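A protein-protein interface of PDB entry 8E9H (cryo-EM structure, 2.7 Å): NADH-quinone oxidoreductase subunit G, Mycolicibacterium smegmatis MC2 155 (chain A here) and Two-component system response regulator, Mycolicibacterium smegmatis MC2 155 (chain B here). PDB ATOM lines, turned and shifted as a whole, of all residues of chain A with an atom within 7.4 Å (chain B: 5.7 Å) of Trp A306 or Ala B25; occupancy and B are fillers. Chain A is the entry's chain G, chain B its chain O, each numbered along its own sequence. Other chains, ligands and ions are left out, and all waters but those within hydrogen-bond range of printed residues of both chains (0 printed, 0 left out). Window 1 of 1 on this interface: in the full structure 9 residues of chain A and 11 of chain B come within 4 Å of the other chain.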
ATOM      1  N   THR A 291      11.095 -12.193   8.579  1.00  0.00           N
ATOM      2  CA  THR A 291      11.881 -13.395   8.357  1.00  0.00           C
ATOM      3  C   THR A 291      11.890 -14.338   9.548  1.00  0.00           C
ATOM      4  O   THR A 291      12.114 -15.539   9.363  1.00  0.00           O
ATOM      5  CB  THR A 291      13.325 -13.022   8.013  1.00  0.00           C
ATOM      6  OG1 THR A 291      13.833 -12.114   8.997  1.00  0.00           O
ATOM      7  CG2 THR A 291      13.393 -12.369   6.645  1.00  0.00           C
ATOM      8  N   THR A 292      11.649 -13.838  10.750  1.00  0.00           N
ATOM      9  CA  THR A 292      11.667 -14.647  11.955  1.00  0.00           C
ATOM     10  C   THR A 292      10.498 -14.240  12.835  1.00  0.00           C
ATOM     11  O   THR A 292      10.000 -13.115  12.730  1.00  0.00           O
ATOM     12  CB  THR A 292      12.977 -14.472  12.733  1.00  0.00           C
ATOM     13  OG1 THR A 292      13.010 -13.171  13.329  1.00  0.00           O
ATOM     14  CG2 THR A 292      14.167 -14.624  11.809  1.00  0.00           C
ATOM     15  N   PRO A 293      10.037 -15.129  13.710  1.00  0.00           N
ATOM     16  CA  PRO A 293       9.011 -14.733  14.676  1.00  0.00           C
ATOM     17  C   PRO A 293       9.506 -13.582  15.536  1.00  0.00           C
ATOM     18  O   PRO A 293      10.677 -13.523  15.914  1.00  0.00           O
ATOM     19  CB  PRO A 293       8.787 -16.004  15.500  1.00  0.00           C
ATOM     20  CG  PRO A 293       9.244 -17.106  14.629  1.00  0.00           C
ATOM     21  CD  PRO A 293      10.375 -16.556  13.828  1.00  0.00           C
ATOM     22  N   ALA A 304      12.466 -13.331  17.824  1.00  0.00           N
ATOM     23  CA  ALA A 304      12.298 -14.361  18.834  1.00  0.00           C
ATOM     24  C   ALA A 304      12.331 -15.726  18.171  1.00  0.00           C
ATOM     25  O   ALA A 304      11.948 -15.879  17.009  1.00  0.00           O
ATOM     26  CB  ALA A 304      10.985 -14.191  19.602  1.00  0.00           C
ATOM     27  N   SER A 305      12.788 -16.718  18.922  1.00  0.00           N
ATOM     28  CA  SER A 305      12.797 -18.082  18.427  1.00  0.00           C
ATOM     29  C   SER A 305      11.370 -18.585  18.248  1.00  0.00           C
ATOM     30  O   SER A 305      10.437 -18.145  18.923  1.00  0.00           O
ATOM     31  CB  SER A 305      13.554 -18.993  19.389  1.00  0.00           C
ATOM     32  OG  SER A 305      12.918 -19.017  20.653  1.00  0.00           O
ATOM     33  N   TRP A 306      11.206 -19.524  17.318  1.00  0.00           N
ATOM     34  CA  TRP A 306       9.884 -20.088  17.084  1.00  0.00           C
ATOM     35  C   TRP A 306       9.294 -20.645  18.368  1.00  0.00           C
ATOM     36  O   TRP A 306       8.101 -20.474  18.636  1.00  0.00           O
ATOM     37  CB  TRP A 306       9.956 -21.179  16.020  1.00  0.00           C
ATOM     38  CG  TRP A 306       9.867 -20.658  14.634  1.00  0.00           C
ATOM     39  CD1 TRP A 306      10.900 -20.399  13.790  1.00  0.00           C
ATOM     40  CD2 TRP A 306       8.673 -20.328  13.924  1.00  0.00           C
ATOM     41  NE1 TRP A 306      10.425 -19.926  12.595  1.00  0.00           N
ATOM     42  CE2 TRP A 306       9.059 -19.874  12.652  1.00  0.00           C
ATOM     43  CE3 TRP A 306       7.315 -20.372  14.240  1.00  0.00           C
ATOM     44  CZ2 TRP A 306       8.136 -19.467  11.697  1.00  0.00           C
ATOM     45  CZ3 TRP A 306       6.403 -19.969  13.293  1.00  0.00           C
ATOM     46  CH2 TRP A 306       6.815 -19.521  12.036  1.00  0.00           C
ATOM     47  N   SER A 307      10.113 -21.312  19.178  1.00  0.00           N
ATOM     48  CA  SER A 307       9.614 -21.880  20.424  1.00  0.00           C
ATOM     49  C   SER A 307       9.121 -20.787  21.363  1.00  0.00           C
ATOM     50  O   SER A 307       8.017 -20.874  21.914  1.00  0.00           O
ATOM     51  CB  SER A 307      10.709 -22.709  21.090  1.00  0.00           C
ATOM     52  OG  SER A 307      10.282 -23.195  22.348  1.00  0.00           O
ATOM     53  N   GLU A 308       9.929 -19.744  21.556  1.00  0.00           N
ATOM     54  CA  GLU A 308       9.538 -18.667  22.457  1.00  0.00           C
ATOM     55  C   GLU A 308       8.282 -17.969  21.956  1.00  0.00           C
ATOM     56  O   GLU A 308       7.363 -17.685  22.733  1.00  0.00           O
ATOM     57  CB  GLU A 308      10.685 -17.669  22.605  1.00  0.00           C
ATOM     58  N   ALA A 309       8.228 -17.679  20.657  1.00  0.00           N
ATOM     59  CA  ALA A 309       7.063 -16.998  20.105  1.00  0.00           C
ATOM     60  C   ALA A 309       5.812 -17.849  20.256  1.00  0.00           C
ATOM     61  O   ALA A 309       4.753 -17.348  20.648  1.00  0.00           O
ATOM     62  CB  ALA A 309       7.304 -16.654  18.637  1.00  0.00           C
ATOM     63  N   LEU A 310       5.914 -19.143  19.952  1.00  0.00           N
ATOM     64  CA  LEU A 310       4.759 -20.018  20.094  1.00  0.00           C
ATOM     65  C   LEU A 310       4.295 -20.076  21.540  1.00  0.00           C
ATOM     66  O   LEU A 310       3.094 -20.016  21.814  1.00  0.00           O
ATOM     67  CB  LEU A 310       5.092 -21.418  19.589  1.00  0.00           C
ATOM     68  CG  LEU A 310       5.089 -21.611  18.076  1.00  0.00           C
ATOM     69  CD1 LEU A 310       5.764 -22.918  17.709  1.00  0.00           C
ATOM     70  CD2 LEU A 310       3.674 -21.581  17.540  1.00  0.00           C
ATOM     71  N   THR A 311       5.231 -20.197  22.481  1.00  0.00           N
ATOM     72  CA  THR A 311       4.849 -20.278  23.885  1.00  0.00           C
ATOM     73  C   THR A 311       4.165 -18.995  24.338  1.00  0.00           C
ATOM     74  O   THR A 311       3.132 -19.036  25.017  1.00  0.00           O
ATOM     75  CB  THR A 311       6.079 -20.564  24.743  1.00  0.00           C
ATOM     76  OG1 THR A 311       6.697 -21.776  24.298  1.00  0.00           O
ATOM     77  CG2 THR A 311       5.690 -20.701  26.202  1.00  0.00           C
ATOM     78  N   VAL A 312       4.725 -17.843  23.970  1.00  0.00           N
ATOM     79  CA  VAL A 312       4.128 -16.577  24.379  1.00  0.00           C
ATOM     80  C   VAL A 312       2.740 -16.427  23.777  1.00  0.00           C
ATOM     81  O   VAL A 312       1.794 -16.006  24.455  1.00  0.00           O
ATOM     82  CB  VAL A 312       5.041 -15.404  23.985  1.00  0.00           C
ATOM     83  CG1 VAL A 312       4.332 -14.086  24.221  1.00  0.00           C
ATOM     84  CG2 VAL A 312       6.334 -15.460  24.769  1.00  0.00           C
ATOM     85  N   VAL A 604       4.413 -11.940  16.395  1.00  0.00           N
ATOM     86  CA  VAL A 604       4.331 -11.926  14.941  1.00  0.00           C
ATOM     87  C   VAL A 604       4.959 -13.206  14.420  1.00  0.00           C
ATOM     88  O   VAL A 604       6.064 -13.572  14.836  1.00  0.00           O
ATOM     89  CB  VAL A 604       5.037 -10.699  14.341  1.00  0.00           C
ATOM     90  CG1 VAL A 604       4.780 -10.627  12.851  1.00  0.00           C
ATOM     91  CG2 VAL A 604       4.574  -9.431  15.032  1.00  0.00           C
ATOM     92  N   PHE A 605       4.259 -13.887  13.521  1.00  0.00           N
ATOM     93  CA  PHE A 605       4.743 -15.128  12.949  1.00  0.00           C
ATOM     94  C   PHE A 605       4.948 -14.973  11.453  1.00  0.00           C
ATOM     95  O   PHE A 605       3.980 -14.700  10.735  1.00  0.00           O
ATOM     96  CB  PHE A 605       3.756 -16.262  13.218  1.00  0.00           C
ATOM     97  CG  PHE A 605       3.673 -16.656  14.656  1.00  0.00           C
ATOM     98  CD1 PHE A 605       4.710 -17.338  15.258  1.00  0.00           C
ATOM     99  CD2 PHE A 605       2.557 -16.348  15.409  1.00  0.00           C
ATOM    100  CE1 PHE A 605       4.637 -17.702  16.580  1.00  0.00           C
ATOM    101  CE2 PHE A 605       2.480 -16.711  16.731  1.00  0.00           C
ATOM    102  CZ  PHE A 605       3.520 -17.388  17.317  1.00  0.00           C
ATOM    103  N   PRO A 606       6.165 -15.139  10.938  1.00  0.00           N
ATOM    104  CA  PRO A 606       6.350 -15.081   9.485  1.00  0.00           C
ATOM    105  C   PRO A 606       5.673 -16.263   8.817  1.00  0.00           C
ATOM    106  O   PRO A 606       5.788 -17.400   9.276  1.00  0.00           O
ATOM    107  CB  PRO A 606       7.871 -15.131   9.320  1.00  0.00           C
ATOM    108  CG  PRO A 606       8.341 -15.861  10.508  1.00  0.00           C
ATOM    109  CD  PRO A 606       7.418 -15.487  11.628  1.00  0.00           C
ATOM    110  N   VAL A 607       4.965 -15.989   7.731  1.00  0.00           N
ATOM    111  CA  VAL A 607       4.225 -17.011   7.007  1.00  0.00           C
ATOM    112  C   VAL A 607       4.652 -16.984   5.550  1.00  0.00           C
ATOM    113  O   VAL A 607       4.971 -15.930   4.990  1.00  0.00           O
ATOM    114  CB  VAL A 607       2.706 -16.807   7.149  1.00  0.00           C
ATOM    115  CG1 VAL A 607       2.299 -16.965   8.602  1.00  0.00           C
ATOM    116  CG2 VAL A 607       2.305 -15.445   6.623  1.00  0.00           C
ATOM    117  N   ASN A 634      12.119 -22.805   3.848  1.00  0.00           N
ATOM    118  CA  ASN A 634      11.741 -23.140   5.216  1.00  0.00           C
ATOM    119  C   ASN A 634      10.497 -22.394   5.674  1.00  0.00           C
ATOM    120  O   ASN A 634       9.938 -22.738   6.720  1.00  0.00           O
ATOM    121  CB  ASN A 634      12.894 -22.838   6.170  1.00  0.00           C
ATOM    122  CG  ASN A 634      13.287 -21.381   6.158  1.00  0.00           C
ATOM    123  OD1 ASN A 634      13.630 -20.828   5.115  1.00  0.00           O
ATOM    124  ND2 ASN A 634      13.237 -20.746   7.320  1.00  0.00           N
ATOM    125  N   ALA A 635      10.054 -21.385   4.930  1.00  0.00           N
ATOM    126  CA  ALA A 635       8.848 -20.667   5.309  1.00  0.00           C
ATOM    127  C   ALA A 635       7.657 -21.616   5.321  1.00  0.00           C
ATOM    128  O   ALA A 635       7.554 -22.530   4.500  1.00  0.00           O
ATOM    129  CB  ALA A 635       8.588 -19.513   4.344  1.00  0.00           C
ATOM    130  N   ILE A 636       6.748 -21.390   6.264  1.00  0.00           N
ATOM    131  CA  ILE A 636       5.622 -22.295   6.472  1.00  0.00           C
ATOM    132  C   ILE A 636       4.311 -21.535   6.318  1.00  0.00           C
ATOM    133  O   ILE A 636       4.260 -20.328   6.591  1.00  0.00           O
ATOM    134  CB  ILE A 636       5.716 -22.973   7.847  1.00  0.00           C
ATOM    135  CG1 ILE A 636       5.659 -21.932   8.963  1.00  0.00           C
ATOM    136  CG2 ILE A 636       6.997 -23.775   7.946  1.00  0.00           C
ATOM    137  CD1 ILE A 636       5.794 -22.523  10.344  1.00  0.00           C
ATOM    138  N   PRO A 637       3.232 -22.189   5.891  1.00  0.00           N
ATOM    139  CA  PRO A 637       1.979 -21.469   5.650  1.00  0.00           C
ATOM    140  C   PRO A 637       1.329 -21.000   6.940  1.00  0.00           C
ATOM    141  O   PRO A 637       1.710 -21.392   8.044  1.00  0.00           O
ATOM    142  CB  PRO A 637       1.099 -22.511   4.947  1.00  0.00           C
ATOM    143  CG  PRO A 637       2.026 -23.578   4.502  1.00  0.00           C
ATOM    144  CD  PRO A 637       3.124 -23.602   5.499  1.00  0.00           C
ATOM    145  N   ARG A 640       0.134 -24.139   8.896  1.00  0.00           N
ATOM    146  CA  ARG A 640       1.031 -24.833   9.812  1.00  0.00           C
ATOM    147  C   ARG A 640       1.316 -24.007  11.056  1.00  0.00           C
ATOM    148  O   ARG A 640       1.427 -24.558  12.157  1.00  0.00           O
ATOM    149  CB  ARG A 640       2.331 -25.184   9.099  1.00  0.00           C
ATOM    150  CG  ARG A 640       2.147 -26.200   7.998  1.00  0.00           C
ATOM    151  CD  ARG A 640       3.468 -26.800   7.594  1.00  0.00           C
ATOM    152  NE  ARG A 640       3.977 -27.702   8.619  1.00  0.00           N
ATOM    153  CZ  ARG A 640       5.259 -27.855   8.914  1.00  0.00           C
ATOM    154  NH1 ARG A 640       6.203 -27.186   8.273  1.00  0.00           N
ATOM    155  NH2 ARG A 640       5.607 -28.703   9.876  1.00  0.00           N
ATOM    156  N   VAL A 641       1.447 -22.690  10.905  1.00  0.00           N
ATOM    157  CA  VAL A 641       1.662 -21.845  12.073  1.00  0.00           C
ATOM    158  C   VAL A 641       0.499 -21.996  13.039  1.00  0.00           C
ATOM    159  O   VAL A 641       0.691 -22.158  14.246  1.00  0.00           O
ATOM    160  CB  VAL A 641       1.857 -20.379  11.653  1.00  0.00           C
ATOM    161  CG1 VAL A 641       1.958 -19.492  12.879  1.00  0.00           C
ATOM    162  CG2 VAL A 641       3.095 -20.236  10.797  1.00  0.00           C
ATOM    163  N   TYR A 644       0.544 -25.579  14.757  1.00  0.00           N
ATOM    164  CA  TYR A 644       1.507 -25.757  15.834  1.00  0.00           C
ATOM    165  C   TYR A 644       1.280 -24.782  16.980  1.00  0.00           C
ATOM    166  O   TYR A 644       1.601 -25.104  18.126  1.00  0.00           O
ATOM    167  CB  TYR A 644       2.921 -25.655  15.274  1.00  0.00           C
ATOM    168  CG  TYR A 644       3.227 -26.839  14.395  1.00  0.00           C
ATOM    169  CD1 TYR A 644       3.224 -28.125  14.917  1.00  0.00           C
ATOM    170  CD2 TYR A 644       3.472 -26.684  13.041  1.00  0.00           C
ATOM    171  CE1 TYR A 644       3.488 -29.216  14.126  1.00  0.00           C
ATOM    172  CE2 TYR A 644       3.737 -27.774  12.238  1.00  0.00           C
ATOM    173  CZ  TYR A 644       3.738 -29.039  12.786  1.00  0.00           C
ATOM    174  OH  TYR A 644       3.999 -30.135  11.997  1.00  0.00           O
ATOM    175  N   GLU B  20      22.022 -19.963  12.470  1.00  0.00           N
ATOM    176  CA  GLU B  20      20.978 -19.042  12.902  1.00  0.00           C
ATOM    177  C   GLU B  20      19.609 -19.703  12.833  1.00  0.00           C
ATOM    178  O   GLU B  20      18.793 -19.566  13.747  1.00  0.00           O
ATOM    179  CB  GLU B  20      21.012 -17.778  12.047  1.00  0.00           C
ATOM    180  N   GLN B  21      19.341 -20.440  11.755  1.00  0.00           N
ATOM    181  CA  GLN B  21      18.055 -21.116  11.632  1.00  0.00           C
ATOM    182  C   GLN B  21      17.884 -22.176  12.710  1.00  0.00           C
ATOM    183  O   GLN B  21      16.796 -22.328  13.271  1.00  0.00           O
ATOM    184  CB  GLN B  21      17.918 -21.745  10.250  1.00  0.00           C
ATOM    185  CG  GLN B  21      17.553 -20.764   9.161  1.00  0.00           C
ATOM    186  CD  GLN B  21      17.600 -21.391   7.788  1.00  0.00           C
ATOM    187  OE1 GLN B  21      17.515 -22.610   7.648  1.00  0.00           O
ATOM    188  NE2 GLN B  21      17.742 -20.560   6.763  1.00  0.00           N
ATOM    189  N   VAL B  22      18.941 -22.933  13.000  1.00  0.00           N
ATOM    190  CA  VAL B  22      18.850 -23.947  14.045  1.00  0.00           C
ATOM    191  C   VAL B  22      18.581 -23.290  15.390  1.00  0.00           C
ATOM    192  O   VAL B  22      17.718 -23.728  16.157  1.00  0.00           O
ATOM    193  CB  VAL B  22      20.129 -24.798  14.082  1.00  0.00           C
ATOM    194  CG1 VAL B  22      20.206 -25.574  15.381  1.00  0.00           C
ATOM    195  CG2 VAL B  22      20.166 -25.741  12.901  1.00  0.00           C
ATOM    196  N   ARG B  23      19.308 -22.229  15.691  1.00  0.00           N
ATOM    197  CA  ARG B  23      19.157 -21.512  16.947  1.00  0.00           C
ATOM    198  C   ARG B  23      17.889 -20.717  17.010  1.00  0.00           C
ATOM    199  O   ARG B  23      17.556 -20.200  18.078  1.00  0.00           O
ATOM    200  CB  ARG B  23      20.366 -20.601  17.148  1.00  0.00           C
ATOM    201  CG  ARG B  23      20.643 -20.243  18.592  1.00  0.00           C
ATOM    202  CD  ARG B  23      22.080 -19.800  18.773  1.00  0.00           C
ATOM    203  NE  ARG B  23      22.395 -18.641  17.947  1.00  0.00           N
ATOM    204  CZ  ARG B  23      23.095 -18.680  16.820  1.00  0.00           C
ATOM    205  NH1 ARG B  23      23.568 -19.817  16.336  1.00  0.00           N
ATOM    206  NH2 ARG B  23      23.320 -17.549  16.159  1.00  0.00           N
ATOM    207  N   LEU B  24      17.188 -20.584  15.895  1.00  0.00           N
ATOM    208  CA  LEU B  24      15.898 -19.914  15.855  1.00  0.00           C
ATOM    209  C   LEU B  24      14.730 -20.871  15.995  1.00  0.00           C
ATOM    210  O   LEU B  24      13.789 -20.581  16.735  1.00  0.00           O
ATOM    211  CB  LEU B  24      15.758 -19.137  14.543  1.00  0.00           C
ATOM    212  CG  LEU B  24      14.533 -18.237  14.435  1.00  0.00           C
ATOM    213  CD1 LEU B  24      14.833 -16.893  15.064  1.00  0.00           C
ATOM    214  CD2 LEU B  24      14.120 -18.078  12.989  1.00  0.00           C
ATOM    215  N   ALA B  25      14.756 -22.003  15.295  1.00  0.00           N
ATOM    216  CA  ALA B  25      13.724 -23.012  15.493  1.00  0.00           C
ATOM    217  C   ALA B  25      13.705 -23.473  16.940  1.00  0.00           C
ATOM    218  O   ALA B  25      12.644 -23.556  17.568  1.00  0.00           O
ATOM    219  CB  ALA B  25      13.963 -24.193  14.558  1.00  0.00           C
ATOM    220  N   LEU B  26      14.875 -23.776  17.484  1.00  0.00           N
ATOM    221  CA  LEU B  26      15.023 -23.989  18.909  1.00  0.00           C
ATOM    222  C   LEU B  26      15.265 -22.652  19.600  1.00  0.00           C
ATOM    223  O   LEU B  26      15.888 -21.744  19.046  1.00  0.00           O
ATOM    224  CB  LEU B  26      16.179 -24.945  19.186  1.00  0.00           C
ATOM    225  CG  LEU B  26      16.299 -26.129  18.228  1.00  0.00           C
ATOM    226  CD1 LEU B  26      17.518 -26.959  18.573  1.00  0.00           C
ATOM    227  CD2 LEU B  26      15.044 -26.974  18.255  1.00  0.00           C
ATOM    228  N   GLY B  27      14.761 -22.536  20.821  1.00  0.00           N
ATOM    229  CA  GLY B  27      14.918 -21.306  21.571  1.00  0.00           C
ATOM    230  C   GLY B  27      15.599 -21.547  22.898  1.00  0.00           C
ATOM    231  O   GLY B  27      16.257 -22.574  23.082  1.00  0.00           O
ATOM    232  N   ILE B 114      15.693 -26.169   6.654  1.00  0.00           N
ATOM    233  CA  ILE B 114      15.373 -26.633   8.000  1.00  0.00           C
ATOM    234  C   ILE B 114      13.968 -26.157   8.348  1.00  0.00           C
ATOM    235  O   ILE B 114      13.744 -24.965   8.569  1.00  0.00           O
ATOM    236  CB  ILE B 114      16.395 -26.133   9.023  1.00  0.00           C
ATOM    237  CG1 ILE B 114      17.817 -26.476   8.573  1.00  0.00           C
ATOM    238  CG2 ILE B 114      16.113 -26.739  10.382  1.00  0.00           C
ATOM    239  CD1 ILE B 114      18.882 -25.725   9.324  1.00  0.00           C
ATOM    240  N   ASP B 115      13.023 -27.082   8.399  1.00  0.00           N
ATOM    241  CA  ASP B 115      11.693 -26.751   8.881  1.00  0.00           C
ATOM    242  C   ASP B 115      11.770 -26.536  10.387  1.00  0.00           C
ATOM    243  O   ASP B 115      12.145 -27.466  11.114  1.00  0.00           O
ATOM    244  CB  ASP B 115      10.710 -27.868   8.554  1.00  0.00           C
ATOM    245  CG  ASP B 115       9.326 -27.616   9.118  1.00  0.00           C
ATOM    246  OD1 ASP B 115       9.147 -26.654   9.892  1.00  0.00           O
ATOM    247  OD2 ASP B 115       8.404 -28.387   8.784  1.00  0.00           O
ATOM    248  N   PRO B 116      11.426 -25.353  10.899  1.00  0.00           N
ATOM    249  CA  PRO B 116      11.609 -25.120  12.338  1.00  0.00           C
ATOM    250  C   PRO B 116      10.874 -26.118  13.203  1.00  0.00           C
ATOM    251  O   PRO B 116      11.431 -26.605  14.196  1.00  0.00           O
ATOM    252  CB  PRO B 116      11.063 -23.701  12.534  1.00  0.00           C
ATOM    253  CG  PRO B 116      11.108 -23.080  11.192  1.00  0.00           C
ATOM    254  CD  PRO B 116      10.842 -24.181  10.229  1.00  0.00           C
ATOM    255  N   ILE B 117       9.642 -26.458  12.841  1.00  0.00           N
ATOM    256  CA  ILE B 117       8.854 -27.351  13.674  1.00  0.00           C
ATOM    257  C   ILE B 117       9.392 -28.769  13.608  1.00  0.00           C
ATOM    258  O   ILE B 117       9.446 -29.469  14.621  1.00  0.00           O
ATOM    259  CB  ILE B 117       7.377 -27.288  13.263  1.00  0.00           C
ATOM    260  CG1 ILE B 117       6.893 -25.836  13.251  1.00  0.00           C
ATOM    261  CG2 ILE B 117       6.554 -28.126  14.207  1.00  0.00           C
ATOM    262  CD1 ILE B 117       7.058 -25.114  14.577  1.00  0.00           C
ATOM    263  N   LEU B 119      12.490 -29.671  13.042  1.00  0.00           N
ATOM    264  CA  LEU B 119      13.714 -29.685  13.830  1.00  0.00           C
ATOM    265  C   LEU B 119      13.400 -29.706  15.318  1.00  0.00           C
ATOM    266  O   LEU B 119      14.004 -30.467  16.082  1.00  0.00           O
ATOM    267  CB  LEU B 119      14.569 -28.471  13.481  1.00  0.00           C
ATOM    268  CG  LEU B 119      15.952 -28.448  14.123  1.00  0.00           C
ATOM    269  CD1 LEU B 119      16.900 -29.350  13.368  1.00  0.00           C
ATOM    270  CD2 LEU B 119      16.481 -27.034  14.170  1.00  0.00           C
ATOM    271  N   SER B 120      12.458 -28.867  15.751  1.00  0.00           N
ATOM    272  CA  SER B 120      12.119 -28.824  17.166  1.00  0.00           C
ATOM    273  C   SER B 120      11.581 -30.167  17.638  1.00  0.00           C
ATOM    274  O   SER B 120      11.949 -30.655  18.712  1.00  0.00           O
ATOM    275  CB  SER B 120      11.100 -27.717  17.421  1.00  0.00           C
ATOM    276  OG  SER B 120      10.829 -27.587  18.803  1.00  0.00           O
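Leu B24 touches Thr A292. O of Ala A304 touches CD1 of Leu B24, at 3.6 Å. Ser A305 touches Leu B24. CB of Ser A305 touches O of Leu B26 (3.6 Å). OG of Ser A305 touches CA of Gly B27, at 3.2 Å. O of Ala B25 touches CB of Trp A306 (3.9 Å). Trp A306 touches Pro B116. O of Ile B114 touches CB of Asn A634 (3.3 Å). Pro B116 touches Asn A634 (CD to O, 3.9 Å). Ile B117 touches Tyr A644.
Hydrophobic or aromatic side chains of chain B within 4 Å of the printed part of chain A: Leu B24, Pro B116 and Ile B117. Of the 23 printed residues of chain A, 8 touch a printed residue of chain B. Hydrophobic or aromatic side chains of chain A that line the printed part of chain B: Trp A306 and Tyr A644. Among the printed residues, Asp or Glu carboxylates within 4 Å of a Lys or Arg side-chain nitrogen of the other chain: Arg A640 with Asp B115.
Val A641 touches none of the printed residues of chain B. Of the printed residues of chain A, Ala B25 touches Trp A306 (3.9 Å) and Ser A307 (3.7 Å). Of the printed residues of chain A, Leu B26 touches Ser A305. Of the printed residues of chain A, Asp B115 touches Arg A640 (2.6 Å). The nearest residue of chain B that does not touch Trp A306 is Ile B117 (4.8 Å). The nearest residue of chain A that does not touch Ala B25 is Ser A305 (5.0 Å). The nearest printed residue of chain A that does not touch Asp B115 is Ile A636 (4.1 Å).
The side-chain carboxylate (OD1) of Asp B115 sits at hydrogen-bond distance from the backbone NH (N) of Ile B117 (3.0 Å). The backbone NH (N) of Ala A304 is in hydrogen-bond range of the backbone carbonyl oxygen (O) of Pro A293 (2.6 Å). OG of Ser A305 is in hydrogen-bond range of N of Glu A308. The backbone carbonyl oxygen (O) of Ser A307 is in hydrogen-bond range of the side-chain hydroxyl (OG1) of Thr A311 (2.9 Å). OH of Tyr A644 is in hydrogen-bond range of NH2 of Arg A640, 3.0 Å away.
O of Leu B24 lies within hydrogen-bond range of N of Trp A306 (2.9 Å). The guanidinium group of Arg A640 lies within salt-bridge range of the side-chain carboxylate of Asp B115.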
